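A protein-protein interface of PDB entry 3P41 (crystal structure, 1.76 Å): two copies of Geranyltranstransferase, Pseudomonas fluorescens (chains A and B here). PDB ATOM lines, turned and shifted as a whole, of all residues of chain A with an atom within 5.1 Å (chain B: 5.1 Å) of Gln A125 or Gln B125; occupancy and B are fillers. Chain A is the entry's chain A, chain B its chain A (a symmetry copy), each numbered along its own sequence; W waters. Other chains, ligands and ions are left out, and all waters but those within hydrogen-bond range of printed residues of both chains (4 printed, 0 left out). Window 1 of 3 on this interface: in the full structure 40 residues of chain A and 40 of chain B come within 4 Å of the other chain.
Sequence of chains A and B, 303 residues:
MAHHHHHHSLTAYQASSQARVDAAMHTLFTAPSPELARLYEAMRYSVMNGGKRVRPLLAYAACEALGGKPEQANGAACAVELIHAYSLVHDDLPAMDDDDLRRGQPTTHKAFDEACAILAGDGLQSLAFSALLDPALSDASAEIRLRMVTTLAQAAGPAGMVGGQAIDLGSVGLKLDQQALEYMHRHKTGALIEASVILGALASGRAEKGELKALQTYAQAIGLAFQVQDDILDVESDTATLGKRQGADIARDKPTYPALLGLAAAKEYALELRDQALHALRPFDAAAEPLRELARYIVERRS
The backbone NH (N) of Ser B126 lies within hydrogen-bond range of the side-chain amide oxygen (OE1) of Gln A125 (3.2 Å). The backbone carbonyl oxygen of Asp A122 is in hydrogen-bond range of the side-chain amide nitrogen of Gln B125, 3.3 Å away. N of Ser A126 lies within hydrogen-bond range of OE1 of Gln B125 (3.2 Å). The side-chain amide nitrogen (NE2) of Gln A125 is in hydrogen-bond range of the backbone carbonyl oxygen (O) of Asp B122, at 3.3 Å. The side-chain carboxylate (OD1) of Asp A122 sits close to the side-chain carboxylate (OD1) of Asp B122, at 3.4 Å.
OH of Tyr B86 is in hydrogen-bond range of NE2 of Gln B125. The side-chain hydroxyl (OH) of Tyr A86 is in hydrogen-bond range of the side-chain amide nitrogen (NE2) of Gln A125 (3.4 Å).
Among the printed residues, merely in contact across the chains: Tyr A86 with Asp B122, Asp A122 with Tyr B86, Gln A125 with Gln B125 and Phe A129 with Phe B129.
Gln A125 touches just these residues of chain B: Asp B122, Gln B125 and Ser B126. Of chain A, only Asp A122, Gln A125 and Ser A126 come within 4 Å of Gln B125. Printed residues of chain B within 4 Å of Asp A122: Tyr B86, Asp B122 and Gln B125. Of the printed residues of chain A, Ser B126 touches Gln A125 (2.4 Å). Printed residues of chain A within 4 Å of Phe B129: Phe A129 (3.7 Å). Of the printed residues of chain B, Tyr A86 touches Asp B122. Printed residues of chain A within 4 Å of Asp B122: Tyr A86, Asp A122 and Gln A125. Ala A128 touches none of the printed residues of chain B. The nearest printed residue of chain B that does not touch Gln A125 is Phe B129 (5.3 Å).
Printed residues of chain A that touch a printed residue of chain B: Tyr A86, Asp A122, Gln A125, Ser A126 and Phe A129. Hydrophobic or aromatic side chains of chain A that line the printed part of chain B: Tyr A86 and Phe A129. Along chain A the printed residues that touch a printed residue of chain B span positions 86 to 129. Among the printed residues, 9 pairs touch across the chains. Among the printed residues, no Asp or Glu carboxylate lies within 4 Å of a Lys or Arg side-chain nitrogen of the other chain.
Tyr A86 touches Asp B122, and with the chains exchanged Asp A122 touches Tyr B86. Asp A122 touches Gln B125, and with the chains exchanged Gln A125 touches Asp B122. Gln A125 touches its own counterpart, Gln B125. Gln A125 touches Ser B126, and with the chains exchanged Ser A126 touches Gln B125. 12 positions are printed for both chains.
Water W1 lies within hydrogen-bond range of OH of Tyr A86 (2.7 Å) and OG of Ser B126 (3.0 Å). Water W4 bridges OH of Tyr B86 (2.7 Å) and OG of Ser A126 (3.0 Å). Water W3 bridges OD2 of Asp B122 (2.9 Å) and OH of Tyr A86 (3.1 Å). Water W2 bridges the side-chain carboxylate of Asp A122 (2.9 Å) and the side-chain hydroxyl of Tyr B86 (3.1 Å).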
ATOM      1  N   LEU A  82      -0.924  15.018  14.901  1.00  0.00           N
ATOM      2  CA  LEU A  82      -1.245  14.027  13.886  1.00  0.00           C
ATOM      3  C   LEU A  82      -1.555  14.728  12.545  1.00  0.00           C
ATOM      4  O   LEU A  82      -1.115  14.259  11.490  1.00  0.00           O
ATOM      5  CB  LEU A  82      -2.446  13.205  14.346  1.00  0.00           C
ATOM      6  CG  LEU A  82      -2.136  12.221  15.463  1.00  0.00           C
ATOM      7  CD1 LEU A  82      -3.417  11.519  15.967  1.00  0.00           C
ATOM      8  CD2 LEU A  82      -1.115  11.213  14.974  1.00  0.00           C
ATOM      9  N   ILE A  83      -2.334  15.812  12.600  1.00  0.00           N
ATOM     10  CA  ILE A  83      -2.512  16.710  11.439  1.00  0.00           C
ATOM     11  C   ILE A  83      -1.173  17.183  10.874  1.00  0.00           C
ATOM     12  O   ILE A  83      -0.908  17.098   9.661  1.00  0.00           O
ATOM     13  CB  ILE A  83      -3.480  17.910  11.703  1.00  0.00           C
ATOM     14  CG1 ILE A  83      -4.901  17.420  12.030  1.00  0.00           C
ATOM     15  CG2 ILE A  83      -3.512  18.842  10.450  1.00  0.00           C
ATOM     16  CD1 ILE A  83      -5.586  16.753  10.853  1.00  0.00           C
ATOM     17  N   TYR A  86       0.596  14.191   9.154  1.00  0.00           N
ATOM     18  CA  TYR A  86       0.001  13.746   7.901  1.00  0.00           C
ATOM     19  C   TYR A  86       0.361  14.756   6.821  1.00  0.00           C
ATOM     20  O   TYR A  86       0.744  14.357   5.712  1.00  0.00           O
ATOM     21  CB  TYR A  86      -1.514  13.554   8.033  1.00  0.00           C
ATOM     22  CG  TYR A  86      -2.338  14.493   7.199  1.00  0.00           C
ATOM     23  CD1 TYR A  86      -2.320  14.426   5.808  1.00  0.00           C
ATOM     24  CD2 TYR A  86      -3.165  15.428   7.803  1.00  0.00           C
ATOM     25  CE1 TYR A  86      -3.094  15.283   5.029  1.00  0.00           C
ATOM     26  CE2 TYR A  86      -3.952  16.277   7.036  1.00  0.00           C
ATOM     27  CZ  TYR A  86      -3.898  16.213   5.661  1.00  0.00           C
ATOM     28  OH  TYR A  86      -4.642  17.081   4.891  1.00  0.00           O
ATOM     29  N   GLY A 121      -0.868   8.987   5.442  1.00  0.00           N
ATOM     30  CA  GLY A 121      -1.281  10.395   5.621  1.00  0.00           C
ATOM     31  C   GLY A 121      -2.796  10.476   5.773  1.00  0.00           C
ATOM     32  O   GLY A 121      -3.328  11.131   6.653  1.00  0.00           O
ATOM     33  N   ASP A 122      -3.511   9.757   4.929  1.00  0.00           N
ATOM     34  CA  ASP A 122      -4.968   9.694   5.022  1.00  0.00           C
ATOM     35  C   ASP A 122      -5.457   9.173   6.389  1.00  0.00           C
ATOM     36  O   ASP A 122      -6.429   9.677   6.950  1.00  0.00           O
ATOM     37  CB  ASP A 122      -5.493   8.831   3.855  1.00  0.00           C
ATOM     38  CG  ASP A 122      -5.391   9.549   2.496  1.00  0.00           C
ATOM     39  OD1 ASP A 122      -5.171  10.790   2.453  1.00  0.00           O
ATOM     40  OD2 ASP A 122      -5.544   8.888   1.461  1.00  0.00           O
ATOM     41  N   GLY A 123      -4.751   8.180   6.916  1.00  0.00           N
ATOM     42  CA  GLY A 123      -5.115   7.475   8.143  1.00  0.00           C
ATOM     43  C   GLY A 123      -4.853   8.374   9.304  1.00  0.00           C
ATOM     44  O   GLY A 123      -5.647   8.480  10.237  1.00  0.00           O
ATOM     45  N   LEU A 124      -3.767   9.126   9.178  1.00  0.00           N
ATOM     46  CA  LEU A 124      -3.376  10.030  10.237  1.00  0.00           C
ATOM     47  C   LEU A 124      -4.357  11.192  10.394  1.00  0.00           C
ATOM     48  O   LEU A 124      -4.622  11.623  11.522  1.00  0.00           O
ATOM     49  CB  LEU A 124      -1.964  10.524   9.968  1.00  0.00           C
ATOM     50  CG  LEU A 124      -0.723   9.744  10.422  1.00  0.00           C
ATOM     51  CD1 LEU A 124       0.571  10.190   9.734  1.00  0.00           C
ATOM     52  CD2 LEU A 124      -0.562   9.645  11.922  1.00  0.00           C
ATOM     53  N   GLN A 125      -4.888  11.720   9.278  1.00  0.00           N
ATOM     54  CA  GLN A 125      -5.903  12.787   9.366  1.00  0.00           C
ATOM     55  C   GLN A 125      -7.134  12.298  10.096  1.00  0.00           C
ATOM     56  O   GLN A 125      -7.683  12.976  10.915  1.00  0.00           O
ATOM     57  CB  GLN A 125      -6.273  13.409   7.997  1.00  0.00           C
ATOM     58  CG  GLN A 125      -7.287  14.531   8.205  1.00  0.00           C
ATOM     59  CD  GLN A 125      -7.766  15.271   6.976  1.00  0.00           C
ATOM     60  OE1 GLN A 125      -8.714  16.046   7.112  1.00  0.00           O
ATOM     61  NE2 GLN A 125      -7.199  15.016   5.793  1.00  0.00           N
ATOM     62  N   SER A 126      -7.586  11.077   9.810  1.00  0.00           N
ATOM     63  CA  SER A 126      -8.695  10.573  10.525  1.00  0.00           C
ATOM     64  C   SER A 126      -8.461  10.357  12.009  1.00  0.00           C
ATOM     65  O   SER A 126      -9.325  10.684  12.830  1.00  0.00           O
ATOM     66  CB  SER A 126      -9.127   9.228   9.888  1.00  0.00           C
ATOM     67  OG  SER A 126      -9.625   9.487   8.596  1.00  0.00           O
ATOM     68  N   LEU A 127      -7.321   9.767  12.348  1.00  0.00           N
ATOM     69  CA  LEU A 127      -6.967   9.487  13.728  1.00  0.00           C
ATOM     70  C   LEU A 127      -6.905  10.784  14.508  1.00  0.00           C
ATOM     71  O   LEU A 127      -7.163  10.797  15.699  1.00  0.00           O
ATOM     72  CB  LEU A 127      -5.595   8.788  13.832  1.00  0.00           C
ATOM     73  CG  LEU A 127      -5.411   7.286  13.686  1.00  0.00           C
ATOM     74  CD1 LEU A 127      -3.941   6.886  13.930  1.00  0.00           C
ATOM     75  CD2 LEU A 127      -6.335   6.568  14.644  1.00  0.00           C
ATOM     76  N   ALA A 128      -6.539  11.863  13.827  1.00  0.00           N
ATOM     77  CA  ALA A 128      -6.440  13.166  14.518  1.00  0.00           C
ATOM     78  C   ALA A 128      -7.809  13.510  15.087  1.00  0.00           C
ATOM     79  O   ALA A 128      -7.933  13.961  16.238  1.00  0.00           O
ATOM     80  CB  ALA A 128      -5.997  14.233  13.541  1.00  0.00           C
ATOM     81  N   PHE A 129      -8.859  13.292  14.291  1.00  0.00           N
ATOM     82  CA  PHE A 129     -10.200  13.564  14.772  1.00  0.00           C
ATOM     83  C   PHE A 129     -10.628  12.547  15.854  1.00  0.00           C
ATOM     84  O   PHE A 129     -11.239  12.917  16.873  1.00  0.00           O
ATOM     85  CB  PHE A 129     -11.213  13.634  13.603  1.00  0.00           C
ATOM     86  CG  PHE A 129     -11.056  14.872  12.736  1.00  0.00           C
ATOM     87  CD1 PHE A 129     -11.585  16.094  13.147  1.00  0.00           C
ATOM     88  CD2 PHE A 129     -10.341  14.821  11.545  1.00  0.00           C
ATOM     89  CE1 PHE A 129     -11.425  17.233  12.372  1.00  0.00           C
ATOM     90  CE2 PHE A 129     -10.154  15.953  10.758  1.00  0.00           C
ATOM     91  CZ  PHE A 129     -10.695  17.171  11.171  1.00  0.00           C
ATOM     92  N   LEU B  82     -18.601  12.943   0.958  1.00  0.00           N
ATOM     93  CA  LEU B  82     -17.325  13.624   0.807  1.00  0.00           C
ATOM     94  C   LEU B  82     -16.167  12.649   1.116  1.00  0.00           C
ATOM     95  O   LEU B  82     -15.158  12.648   0.403  1.00  0.00           O
ATOM     96  CB  LEU B  82     -17.278  14.820   1.754  1.00  0.00           C
ATOM     97  CG  LEU B  82     -18.153  15.988   1.328  1.00  0.00           C
ATOM     98  CD1 LEU B  82     -18.158  17.108   2.393  1.00  0.00           C
ATOM     99  CD2 LEU B  82     -17.673  16.510  -0.014  1.00  0.00           C
ATOM    100  N   ILE B  83     -16.313  11.864   2.188  1.00  0.00           N
ATOM    101  CA  ILE B  83     -15.404  10.730   2.459  1.00  0.00           C
ATOM    102  C   ILE B  83     -15.297   9.787   1.260  1.00  0.00           C
ATOM    103  O   ILE B  83     -14.195   9.429   0.806  1.00  0.00           O
ATOM    104  CB  ILE B  83     -15.732   9.950   3.775  1.00  0.00           C
ATOM    105  CG1 ILE B  83     -15.592  10.855   5.010  1.00  0.00           C
ATOM    106  CG2 ILE B  83     -14.779   8.719   3.905  1.00  0.00           C
ATOM    107  CD1 ILE B  83     -14.161  11.280   5.277  1.00  0.00           C
ATOM    108  N   TYR B  86     -13.334  11.568  -1.572  1.00  0.00           N
ATOM    109  CA  TYR B  86     -11.908  11.743  -1.331  1.00  0.00           C
ATOM    110  C   TYR B  86     -11.227  10.396  -1.521  1.00  0.00           C
ATOM    111  O   TYR B  86     -10.172  10.328  -2.168  1.00  0.00           O
ATOM    112  CB  TYR B  86     -11.637  12.339   0.054  1.00  0.00           C
ATOM    113  CG  TYR B  86     -10.900  11.429   0.994  1.00  0.00           C
ATOM    114  CD1 TYR B  86      -9.578  11.061   0.751  1.00  0.00           C
ATOM    115  CD2 TYR B  86     -11.513  10.961   2.146  1.00  0.00           C
ATOM    116  CE1 TYR B  86      -8.883  10.230   1.627  1.00  0.00           C
ATOM    117  CE2 TYR B  86     -10.824  10.144   3.033  1.00  0.00           C
ATOM    118  CZ  TYR B  86      -9.528   9.769   2.760  1.00  0.00           C
ATOM    119  OH  TYR B  86      -8.850   8.923   3.611  1.00  0.00           O
ATOM    120  N   GLY B 121      -8.205  15.583  -2.329  1.00  0.00           N
ATOM    121  CA  GLY B 121      -8.632  14.448  -1.484  1.00  0.00           C
ATOM    122  C   GLY B 121      -8.449  14.798  -0.013  1.00  0.00           C
ATOM    123  O   GLY B 121      -9.318  14.599   0.819  1.00  0.00           O
ATOM    124  N   ASP B 122      -7.312  15.381   0.317  1.00  0.00           N
ATOM    125  CA  ASP B 122      -7.050  15.832   1.683  1.00  0.00           C
ATOM    126  C   ASP B 122      -8.094  16.850   2.185  1.00  0.00           C
ATOM    127  O   ASP B 122      -8.526  16.801   3.335  1.00  0.00           O
ATOM    128  CB  ASP B 122      -5.615  16.399   1.741  1.00  0.00           C
ATOM    129  CG  ASP B 122      -4.541  15.300   1.664  1.00  0.00           C
ATOM    130  OD1 ASP B 122      -4.860  14.091   1.829  1.00  0.00           O
ATOM    131  OD2 ASP B 122      -3.365  15.630   1.454  1.00  0.00           O
ATOM    132  N   GLY B 123      -8.503  17.746   1.295  1.00  0.00           N
ATOM    133  CA  GLY B 123      -9.397  18.859   1.602  1.00  0.00           C
ATOM    134  C   GLY B 123     -10.774  18.323   1.802  1.00  0.00           C
ATOM    135  O   GLY B 123     -11.497  18.709   2.719  1.00  0.00           O
ATOM    136  N   LEU B 124     -11.092  17.322   0.991  1.00  0.00           N
ATOM    137  CA  LEU B 124     -12.404  16.716   1.055  1.00  0.00           C
ATOM    138  C   LEU B 124     -12.619  15.942   2.356  1.00  0.00           C
ATOM    139  O   LEU B 124     -13.727  15.957   2.903  1.00  0.00           O
ATOM    140  CB  LEU B 124     -12.597  15.827  -0.162  1.00  0.00           C
ATOM    141  CG  LEU B 124     -13.113  16.371  -1.501  1.00  0.00           C
ATOM    142  CD1 LEU B 124     -12.872  15.428  -2.684  1.00  0.00           C
ATOM    143  CD2 LEU B 124     -14.536  16.880  -1.462  1.00  0.00           C
ATOM    144  N   GLN B 125     -11.579  15.249   2.853  1.00  0.00           N
ATOM    145  CA  GLN B 125     -11.697  14.549   4.146  1.00  0.00           C
ATOM    146  C   GLN B 125     -11.979  15.530   5.263  1.00  0.00           C
ATOM    147  O   GLN B 125     -12.794  15.295   6.106  1.00  0.00           O
ATOM    148  CB  GLN B 125     -10.481  13.653   4.482  1.00  0.00           C
ATOM    149  CG  GLN B 125     -10.725  12.940   5.809  1.00  0.00           C
ATOM    150  CD  GLN B 125      -9.644  12.004   6.305  1.00  0.00           C
ATOM    151  OE1 GLN B 125      -9.750  11.571   7.453  1.00  0.00           O
ATOM    152  NE2 GLN B 125      -8.597  11.735   5.519  1.00  0.00           N
ATOM    153  N   SER B 126     -11.302  16.678   5.274  1.00  0.00           N
ATOM    154  CA  SER B 126     -11.595  17.637   6.267  1.00  0.00           C
ATOM    155  C   SER B 126     -12.990  18.230   6.201  1.00  0.00           C
ATOM    156  O   SER B 126     -13.648  18.396   7.235  1.00  0.00           O
ATOM    157  CB  SER B 126     -10.561  18.787   6.169  1.00  0.00           C
ATOM    158  OG  SER B 126      -9.296  18.279   6.526  1.00  0.00           O
ATOM    159  N   LEU B 127     -13.422  18.590   4.997  1.00  0.00           N
ATOM    160  CA  LEU B 127     -14.732  19.180   4.782  1.00  0.00           C
ATOM    161  C   LEU B 127     -15.805  18.210   5.235  1.00  0.00           C
ATOM    162  O   LEU B 127     -16.869  18.626   5.657  1.00  0.00           O
ATOM    163  CB  LEU B 127     -14.968  19.510   3.294  1.00  0.00           C
ATOM    164  CG  LEU B 127     -14.496  20.800   2.640  1.00  0.00           C
ATOM    165  CD1 LEU B 127     -14.963  20.874   1.171  1.00  0.00           C
ATOM    166  CD2 LEU B 127     -15.007  21.983   3.432  1.00  0.00           C
ATOM    167  N   ALA B 128     -15.517  16.920   5.119  1.00  0.00           N
ATOM    168  CA  ALA B 128     -16.516  15.908   5.526  1.00  0.00           C
ATOM    169  C   ALA B 128     -16.825  16.109   7.002  1.00  0.00           C
ATOM    170  O   ALA B 128     -17.993  16.077   7.426  1.00  0.00           O
ATOM    171  CB  ALA B 128     -15.965  14.519   5.291  1.00  0.00           C
ATOM    172  N   PHE B 129     -15.781  16.329   7.807  1.00  0.00           N
ATOM    173  CA  PHE B 129     -15.996  16.562   9.222  1.00  0.00           C
ATOM    174  C   PHE B 129     -16.662  17.934   9.474  1.00  0.00           C
ATOM    175  O   PHE B 129     -17.572  18.058  10.312  1.00  0.00           O
ATOM    176  CB  PHE B 129     -14.681  16.394  10.024  1.00  0.00           C
ATOM    177  CG  PHE B 129     -14.211  14.952  10.127  1.00  0.00           C
ATOM    178  CD1 PHE B 129     -14.784  14.088  11.058  1.00  0.00           C
ATOM    179  CD2 PHE B 129     -13.241  14.457   9.263  1.00  0.00           C
ATOM    180  CE1 PHE B 129     -14.376  12.764  11.141  1.00  0.00           C
ATOM    181  CE2 PHE B 129     -12.827  13.130   9.317  1.00  0.00           C
ATOM    182  CZ  PHE B 129     -13.397  12.272  10.258  1.00  0.00           C
HETATM  183  O   HOH W   1      -6.333  18.714   6.196  1.00  0.00           O
HETATM  184  O   HOH W   2      -7.731   6.986   1.443  1.00  0.00           O
HETATM  185  O   HOH W   3      -2.373  17.919   2.927  1.00  0.00           O
HETATM  186  O   HOH W   4     -10.100   8.244   5.892  1.00  0.00           O
